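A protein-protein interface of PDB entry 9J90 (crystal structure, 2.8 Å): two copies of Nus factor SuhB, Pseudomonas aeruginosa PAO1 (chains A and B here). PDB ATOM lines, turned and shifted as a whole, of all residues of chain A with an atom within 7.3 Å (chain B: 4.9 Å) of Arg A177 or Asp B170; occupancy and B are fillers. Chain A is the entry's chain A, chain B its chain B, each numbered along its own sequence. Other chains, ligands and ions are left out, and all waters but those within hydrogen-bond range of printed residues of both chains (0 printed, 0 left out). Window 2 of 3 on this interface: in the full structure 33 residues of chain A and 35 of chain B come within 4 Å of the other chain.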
ATOM      1  N   ASN A 171     -27.220  18.065  18.521  1.00  0.00           N
ATOM      2  CA  ASN A 171     -26.249  17.561  17.526  1.00  0.00           C
ATOM      3  C   ASN A 171     -25.020  17.011  18.223  1.00  0.00           C
ATOM      4  O   ASN A 171     -24.614  15.858  17.961  1.00  0.00           O
ATOM      5  CB  ASN A 171     -25.890  18.621  16.492  1.00  0.00           C
ATOM      6  CG  ASN A 171     -27.038  18.931  15.565  1.00  0.00           C
ATOM      7  OD1 ASN A 171     -26.813  19.319  14.423  1.00  0.00           O
ATOM      8  ND2 ASN A 171     -28.262  18.771  16.040  1.00  0.00           N
ATOM      9  N   TYR A 172     -24.464  17.793  19.121  1.00  0.00           N
ATOM     10  CA  TYR A 172     -23.308  17.365  19.927  1.00  0.00           C
ATOM     11  C   TYR A 172     -23.583  16.038  20.614  1.00  0.00           C
ATOM     12  O   TYR A 172     -22.802  15.087  20.473  1.00  0.00           O
ATOM     13  CB  TYR A 172     -22.965  18.479  20.924  1.00  0.00           C
ATOM     14  CG  TYR A 172     -21.751  18.175  21.755  1.00  0.00           C
ATOM     15  CD1 TYR A 172     -20.512  18.008  21.146  1.00  0.00           C
ATOM     16  CD2 TYR A 172     -21.840  18.004  23.124  1.00  0.00           C
ATOM     17  CE1 TYR A 172     -19.382  17.711  21.887  1.00  0.00           C
ATOM     18  CE2 TYR A 172     -20.722  17.703  23.878  1.00  0.00           C
ATOM     19  CZ  TYR A 172     -19.493  17.541  23.255  1.00  0.00           C
ATOM     20  OH  TYR A 172     -18.386  17.210  23.976  1.00  0.00           O
ATOM     21  N   LEU A 173     -24.691  15.958  21.327  1.00  0.00           N
ATOM     22  CA  LEU A 173     -24.986  14.732  22.101  1.00  0.00           C
ATOM     23  C   LEU A 173     -25.197  13.570  21.151  1.00  0.00           C
ATOM     24  O   LEU A 173     -24.934  12.427  21.531  1.00  0.00           O
ATOM     25  CB  LEU A 173     -26.196  15.016  22.987  1.00  0.00           C
ATOM     26  CG  LEU A 173     -25.901  16.050  24.073  1.00  0.00           C
ATOM     27  CD1 LEU A 173     -27.171  16.645  24.645  1.00  0.00           C
ATOM     28  CD2 LEU A 173     -25.039  15.433  25.164  1.00  0.00           C
ATOM     29  N   ASN A 174     -25.628  13.853  19.927  1.00  0.00           N
ATOM     30  CA  ASN A 174     -25.697  12.767  18.927  1.00  0.00           C
ATOM     31  C   ASN A 174     -24.292  12.324  18.536  1.00  0.00           C
ATOM     32  O   ASN A 174     -24.007  11.127  18.605  1.00  0.00           O
ATOM     33  CB  ASN A 174     -26.602  13.115  17.754  1.00  0.00           C
ATOM     34  CG  ASN A 174     -28.048  13.102  18.188  1.00  0.00           C
ATOM     35  OD1 ASN A 174     -28.444  12.286  19.027  1.00  0.00           O
ATOM     36  ND2 ASN A 174     -28.808  14.049  17.675  1.00  0.00           N
ATOM     37  N   MET A 175     -23.424  13.278  18.213  1.00  0.00           N
ATOM     38  CA  MET A 175     -22.005  12.960  17.940  1.00  0.00           C
ATOM     39  C   MET A 175     -21.439  12.106  19.066  1.00  0.00           C
ATOM     40  O   MET A 175     -21.070  10.943  18.855  1.00  0.00           O
ATOM     41  CB  MET A 175     -21.126  14.201  17.774  1.00  0.00           C
ATOM     42  CG  MET A 175     -21.332  14.903  16.447  1.00  0.00           C
ATOM     43  SD  MET A 175     -20.577  16.540  16.480  1.00  0.00           S
ATOM     44  CE  MET A 175     -21.631  17.514  15.401  1.00  0.00           C
ATOM     45  N   PHE A 176     -21.456  12.659  20.266  1.00  0.00           N
ATOM     46  CA  PHE A 176     -21.019  11.976  21.504  1.00  0.00           C
ATOM     47  C   PHE A 176     -21.560  10.547  21.541  1.00  0.00           C
ATOM     48  O   PHE A 176     -20.752   9.614  21.749  1.00  0.00           O
ATOM     49  CB  PHE A 176     -21.498  12.806  22.696  1.00  0.00           C
ATOM     50  CG  PHE A 176     -21.014  12.382  24.050  1.00  0.00           C
ATOM     51  CD1 PHE A 176     -21.707  11.433  24.780  1.00  0.00           C
ATOM     52  CD2 PHE A 176     -19.906  12.976  24.623  1.00  0.00           C
ATOM     53  CE1 PHE A 176     -21.291  11.067  26.054  1.00  0.00           C
ATOM     54  CE2 PHE A 176     -19.485  12.606  25.894  1.00  0.00           C
ATOM     55  CZ  PHE A 176     -20.182  11.658  26.612  1.00  0.00           C
ATOM     56  N   ARG A 177     -22.854  10.383  21.312  1.00  0.00           N
ATOM     57  CA  ARG A 177     -23.469   9.058  21.476  1.00  0.00           C
ATOM     58  C   ARG A 177     -22.850   8.062  20.544  1.00  0.00           C
ATOM     59  O   ARG A 177     -22.616   6.940  20.974  1.00  0.00           O
ATOM     60  CB  ARG A 177     -24.965   9.286  21.201  1.00  0.00           C
ATOM     61  CG  ARG A 177     -25.939   8.157  21.513  1.00  0.00           C
ATOM     62  CD  ARG A 177     -27.349   8.591  21.109  1.00  0.00           C
ATOM     63  NE  ARG A 177     -28.462   7.777  21.589  1.00  0.00           N
ATOM     64  CZ  ARG A 177     -28.759   6.547  21.152  1.00  0.00           C
ATOM     65  NH1 ARG A 177     -28.002   5.950  20.249  1.00  0.00           N
ATOM     66  NH2 ARG A 177     -29.831   5.909  21.605  1.00  0.00           N
ATOM     67  N   SER A 178     -22.621   8.446  19.298  1.00  0.00           N
ATOM     68  CA  SER A 178     -22.101   7.499  18.296  1.00  0.00           C
ATOM     69  C   SER A 178     -20.671   7.074  18.649  1.00  0.00           C
ATOM     70  O   SER A 178     -20.265   5.933  18.284  1.00  0.00           O
ATOM     71  CB  SER A 178     -22.234   8.044  16.890  1.00  0.00           C
ATOM     72  OG  SER A 178     -21.325   9.103  16.648  1.00  0.00           O
ATOM     73  N   LEU A 179     -19.981   7.868  19.463  1.00  0.00           N
ATOM     74  CA  LEU A 179     -18.557   7.628  19.735  1.00  0.00           C
ATOM     75  C   LEU A 179     -18.396   6.724  20.962  1.00  0.00           C
ATOM     76  O   LEU A 179     -17.313   6.215  21.255  1.00  0.00           O
ATOM     77  CB  LEU A 179     -17.842   8.960  19.926  1.00  0.00           C
ATOM     78  CG  LEU A 179     -17.604   9.733  18.630  1.00  0.00           C
ATOM     79  CD1 LEU A 179     -17.210  11.176  18.883  1.00  0.00           C
ATOM     80  CD2 LEU A 179     -16.541   9.062  17.792  1.00  0.00           C
ATOM     81  N   VAL A 180     -19.483   6.570  21.704  1.00  0.00           N
ATOM     82  CA  VAL A 180     -19.402   5.940  23.047  1.00  0.00           C
ATOM     83  C   VAL A 180     -19.087   4.449  22.931  1.00  0.00           C
ATOM     84  O   VAL A 180     -18.338   3.936  23.781  1.00  0.00           O
ATOM     85  CB  VAL A 180     -20.597   6.256  23.972  1.00  0.00           C
ATOM     86  CG1 VAL A 180     -20.657   5.299  25.154  1.00  0.00           C
ATOM     87  CG2 VAL A 180     -20.539   7.689  24.493  1.00  0.00           C
ATOM     88  N   GLY A 181     -19.569   3.770  21.902  1.00  0.00           N
ATOM     89  CA  GLY A 181     -19.387   2.316  21.798  1.00  0.00           C
ATOM     90  C   GLY A 181     -17.942   1.901  21.625  1.00  0.00           C
ATOM     91  O   GLY A 181     -17.435   1.051  22.400  1.00  0.00           O
ATOM     92  N   GLN A 182     -17.257   2.527  20.672  1.00  0.00           N
ATOM     93  CA  GLN A 182     -15.889   2.110  20.291  1.00  0.00           C
ATOM     94  C   GLN A 182     -14.883   2.585  21.334  1.00  0.00           C
ATOM     95  O   GLN A 182     -13.975   1.813  21.704  1.00  0.00           O
ATOM     96  CB  GLN A 182     -15.426   2.630  18.929  1.00  0.00           C
ATOM     97  CG  GLN A 182     -16.457   2.566  17.824  1.00  0.00           C
ATOM     98  CD  GLN A 182     -17.298   3.819  17.799  1.00  0.00           C
ATOM     99  OE1 GLN A 182     -18.047   4.088  18.741  1.00  0.00           O
ATOM    100  NE2 GLN A 182     -17.172   4.601  16.732  1.00  0.00           N
ATOM    101  N   ILE A 186     -14.294   9.221  26.695  1.00  0.00           N
ATOM    102  CA  ILE A 186     -14.291  10.640  26.290  1.00  0.00           C
ATOM    103  C   ILE A 186     -14.023  11.466  27.546  1.00  0.00           C
ATOM    104  O   ILE A 186     -14.635  11.224  28.574  1.00  0.00           O
ATOM    105  CB  ILE A 186     -15.614  10.967  25.589  1.00  0.00           C
ATOM    106  CG1 ILE A 186     -15.864   9.935  24.496  1.00  0.00           C
ATOM    107  CG2 ILE A 186     -15.581  12.394  25.064  1.00  0.00           C
ATOM    108  CD1 ILE A 186     -17.218  10.006  23.904  1.00  0.00           C
ATOM    109  N   TRP A 208     -12.520  16.670  19.335  1.00  0.00           N
ATOM    110  CA  TRP A 208     -13.423  17.524  18.534  1.00  0.00           C
ATOM    111  C   TRP A 208     -14.180  18.443  19.460  1.00  0.00           C
ATOM    112  O   TRP A 208     -14.564  18.010  20.541  1.00  0.00           O
ATOM    113  CB  TRP A 208     -14.384  16.667  17.718  1.00  0.00           C
ATOM    114  CG  TRP A 208     -15.697  16.370  18.382  1.00  0.00           C
ATOM    115  CD1 TRP A 208     -16.899  16.981  18.151  1.00  0.00           C
ATOM    116  CD2 TRP A 208     -15.954  15.352  19.362  1.00  0.00           C
ATOM    117  NE1 TRP A 208     -17.877  16.422  18.923  1.00  0.00           N
ATOM    118  CE2 TRP A 208     -17.337  15.404  19.660  1.00  0.00           C
ATOM    119  CE3 TRP A 208     -15.159  14.400  20.000  1.00  0.00           C
ATOM    120  CZ2 TRP A 208     -17.932  14.572  20.602  1.00  0.00           C
ATOM    121  CZ3 TRP A 208     -15.759  13.569  20.930  1.00  0.00           C
ATOM    122  CH2 TRP A 208     -17.121  13.657  21.227  1.00  0.00           C
ATOM    123  N   THR A 260     -17.181   9.804  11.484  1.00  0.00           N
ATOM    124  CA  THR A 260     -18.246   9.520  12.469  1.00  0.00           C
ATOM    125  C   THR A 260     -19.148  10.742  12.640  1.00  0.00           C
ATOM    126  O   THR A 260     -20.379  10.581  12.749  1.00  0.00           O
ATOM    127  CB  THR A 260     -17.674   8.965  13.773  1.00  0.00           C
ATOM    128  OG1 THR A 260     -16.971   7.784  13.391  1.00  0.00           O
ATOM    129  CG2 THR A 260     -18.738   8.638  14.796  1.00  0.00           C
ATOM    130  N   HIS A 264     -24.124  13.751  11.475  1.00  0.00           N
ATOM    131  CA  HIS A 264     -24.795  14.664  12.426  1.00  0.00           C
ATOM    132  C   HIS A 264     -24.527  16.133  12.087  1.00  0.00           C
ATOM    133  O   HIS A 264     -24.801  16.977  12.947  1.00  0.00           O
ATOM    134  CB  HIS A 264     -24.366  14.351  13.872  1.00  0.00           C
ATOM    135  CG  HIS A 264     -24.458  12.905  14.241  1.00  0.00           C
ATOM    136  ND1 HIS A 264     -25.654  12.315  14.539  1.00  0.00           N
ATOM    137  CD2 HIS A 264     -23.512  11.937  14.328  1.00  0.00           C
ATOM    138  CE1 HIS A 264     -25.449  11.036  14.817  1.00  0.00           C
ATOM    139  NE2 HIS A 264     -24.136  10.774  14.699  1.00  0.00           N
ATOM    140  N   ILE B 166     -28.662   1.167  24.370  1.00  0.00           N
ATOM    141  CA  ILE B 166     -28.547   2.573  24.865  1.00  0.00           C
ATOM    142  C   ILE B 166     -29.175   2.673  26.273  1.00  0.00           C
ATOM    143  O   ILE B 166     -29.671   3.772  26.623  1.00  0.00           O
ATOM    144  CB  ILE B 166     -29.166   3.588  23.865  1.00  0.00           C
ATOM    145  CG1 ILE B 166     -29.191   3.108  22.401  1.00  0.00           C
ATOM    146  CG2 ILE B 166     -28.443   4.922  24.016  1.00  0.00           C
ATOM    147  CD1 ILE B 166     -30.579   2.887  21.793  1.00  0.00           C
ATOM    148  N   ASP B 167     -29.089   1.598  27.069  1.00  0.00           N
ATOM    149  CA  ASP B 167     -29.880   1.394  28.316  1.00  0.00           C
ATOM    150  C   ASP B 167     -29.504   2.501  29.295  1.00  0.00           C
ATOM    151  O   ASP B 167     -30.324   3.406  29.515  1.00  0.00           O
ATOM    152  CB  ASP B 167     -29.655   0.007  28.933  1.00  0.00           C
ATOM    153  CG  ASP B 167     -28.623  -0.838  28.203  1.00  0.00           C
ATOM    154  OD1 ASP B 167     -29.013  -1.475  27.202  1.00  0.00           O
ATOM    155  OD2 ASP B 167     -27.432  -0.825  28.613  1.00  0.00           O
ATOM    156  N   ASN B 168     -28.292   2.416  29.831  1.00  0.00           N
ATOM    157  CA  ASN B 168     -27.717   3.436  30.744  1.00  0.00           C
ATOM    158  C   ASN B 168     -27.605   4.738  29.961  1.00  0.00           C
ATOM    159  O   ASN B 168     -28.038   5.774  30.422  1.00  0.00           O
ATOM    160  CB  ASN B 168     -26.337   3.026  31.267  1.00  0.00           C
ATOM    161  CG  ASN B 168     -26.332   1.640  31.869  1.00  0.00           C
ATOM    162  OD1 ASN B 168     -25.308   1.196  32.384  1.00  0.00           O
ATOM    163  ND2 ASN B 168     -27.467   0.960  31.826  1.00  0.00           N
ATOM    164  N   LEU B 169     -26.928   4.649  28.815  1.00  0.00           N
ATOM    165  CA  LEU B 169     -26.454   5.810  28.025  1.00  0.00           C
ATOM    166  C   LEU B 169     -27.487   6.932  27.971  1.00  0.00           C
ATOM    167  O   LEU B 169     -27.174   8.059  28.442  1.00  0.00           O
ATOM    168  CB  LEU B 169     -26.045   5.319  26.634  1.00  0.00           C
ATOM    169  CG  LEU B 169     -25.464   6.384  25.708  1.00  0.00           C
ATOM    170  CD1 LEU B 169     -24.419   7.220  26.443  1.00  0.00           C
ATOM    171  CD2 LEU B 169     -24.878   5.746  24.455  1.00  0.00           C
ATOM    172  N   ASP B 170     -28.665   6.648  27.432  1.00  0.00           N
ATOM    173  CA  ASP B 170     -29.767   7.621  27.369  1.00  0.00           C
ATOM    174  C   ASP B 170     -29.970   8.333  28.697  1.00  0.00           C
ATOM    175  O   ASP B 170     -29.969   9.605  28.710  1.00  0.00           O
ATOM    176  CB  ASP B 170     -31.066   6.970  26.891  1.00  0.00           C
ATOM    177  CG  ASP B 170     -31.358   7.415  25.474  1.00  0.00           C
ATOM    178  OD1 ASP B 170     -30.473   7.147  24.623  1.00  0.00           O
ATOM    179  OD2 ASP B 170     -32.403   8.105  25.259  1.00  0.00           O
ATOM    180  N   ASN B 171     -30.160   7.531  29.756  1.00  0.00           N
ATOM    181  CA  ASN B 171     -30.418   8.085  31.104  1.00  0.00           C
ATOM    182  C   ASN B 171     -29.482   9.249  31.459  1.00  0.00           C
ATOM    183  O   ASN B 171     -29.967  10.252  32.060  1.00  0.00           O
ATOM    184  CB  ASN B 171     -30.232   6.986  32.165  1.00  0.00           C
ATOM    185  CG  ASN B 171     -31.206   5.835  32.032  1.00  0.00           C
ATOM    186  OD1 ASN B 171     -30.854   4.684  32.282  1.00  0.00           O
ATOM    187  ND2 ASN B 171     -32.429   6.143  31.638  1.00  0.00           N
ATOM    188  N   TYR B 172     -28.199   8.983  31.299  1.00  0.00           N
ATOM    189  CA  TYR B 172     -27.148   9.931  31.674  1.00  0.00           C
ATOM    190  C   TYR B 172     -27.280  11.153  30.784  1.00  0.00           C
ATOM    191  O   TYR B 172     -27.257  12.295  31.268  1.00  0.00           O
ATOM    192  CB  TYR B 172     -25.800   9.204  31.662  1.00  0.00           C
ATOM    193  CG  TYR B 172     -24.548  10.037  31.512  1.00  0.00           C
ATOM    194  CD1 TYR B 172     -24.217  10.584  30.279  1.00  0.00           C
ATOM    195  CD2 TYR B 172     -23.628  10.165  32.547  1.00  0.00           C
ATOM    196  CE1 TYR B 172     -23.051  11.305  30.094  1.00  0.00           C
ATOM    197  CE2 TYR B 172     -22.451  10.877  32.374  1.00  0.00           C
ATOM    198  CZ  TYR B 172     -22.161  11.446  31.140  1.00  0.00           C
ATOM    199  OH  TYR B 172     -21.017  12.156  30.900  1.00  0.00           O
ATOM    200  N   LEU B 173     -27.392  10.906  29.486  1.00  0.00           N
ATOM    201  CA  LEU B 173     -27.369  12.010  28.499  1.00  0.00           C
ATOM    202  C   LEU B 173     -28.576  12.903  28.742  1.00  0.00           C
ATOM    203  O   LEU B 173     -28.484  14.123  28.461  1.00  0.00           O
ATOM    204  CB  LEU B 173     -27.362  11.474  27.065  1.00  0.00           C
ATOM    205  CG  LEU B 173     -26.097  10.745  26.609  1.00  0.00           C
ATOM    206  CD1 LEU B 173     -26.277  10.217  25.197  1.00  0.00           C
ATOM    207  CD2 LEU B 173     -24.865  11.638  26.664  1.00  0.00           C
ATOM    208  N   ASN B 174     -29.658  12.355  29.271  1.00  0.00           N
ATOM    209  CA  ASN B 174     -30.801  13.213  29.610  1.00  0.00           C
ATOM    210  C   ASN B 174     -30.442  14.102  30.800  1.00  0.00           C
ATOM    211  O   ASN B 174     -30.615  15.344  30.698  1.00  0.00           O
ATOM    212  CB  ASN B 174     -32.073  12.367  29.713  1.00  0.00           C
ATOM    213  CG  ASN B 174     -32.674  12.138  28.341  1.00  0.00           C
ATOM    214  OD1 ASN B 174     -32.942  13.105  27.635  1.00  0.00           O
ATOM    215  ND2 ASN B 174     -32.898  10.885  27.956  1.00  0.00           N
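Among the printed residues, merely in contact across the chains: Arg A177 with Ile B166, Phe A176 with Leu B173 and Arg A177 with Leu B169.
Of the 9 printed residues of chain B, 4 touch a printed residue of chain A. Printed residues of chain B that touch a printed residue of chain A: Ile B166, Leu B169, Asp B170 and Leu B173. Among the printed residues, Asp or Glu carboxylates within 4 Å of a Lys or Arg side-chain nitrogen of the other chain: Arg A177 with Asp B170.
The guanidinium group (NH2) of Arg A177 is in salt-bridge range of the side-chain carboxylate (OD1) of Asp B170 (3.3 Å).
The backbone carbonyl oxygen (O) of Asp B170 is in hydrogen-bond range of the side-chain amide nitrogen (ND2) of Asn B174.
4 positions are printed for both chains.
Printed residues of chain B within 4 Å of Phe A176: Leu B173 (3.7 Å). Printed residues of chain A within 4 Å of Ile B166: Arg A177 (3.0 Å). Of the printed residues of chain A, Leu B169 touches Arg A177 (3.9 Å). Asp B170 touches one residue of chain A. Of the printed residues of chain A, Leu B173 touches Phe A176. The nearest printed residue of chain A that does not touch Asp B170 is Asn A174 (7.9 Å). The nearest printed residue of chain A that does not touch Leu B173 is Leu A173 (4.1 Å).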
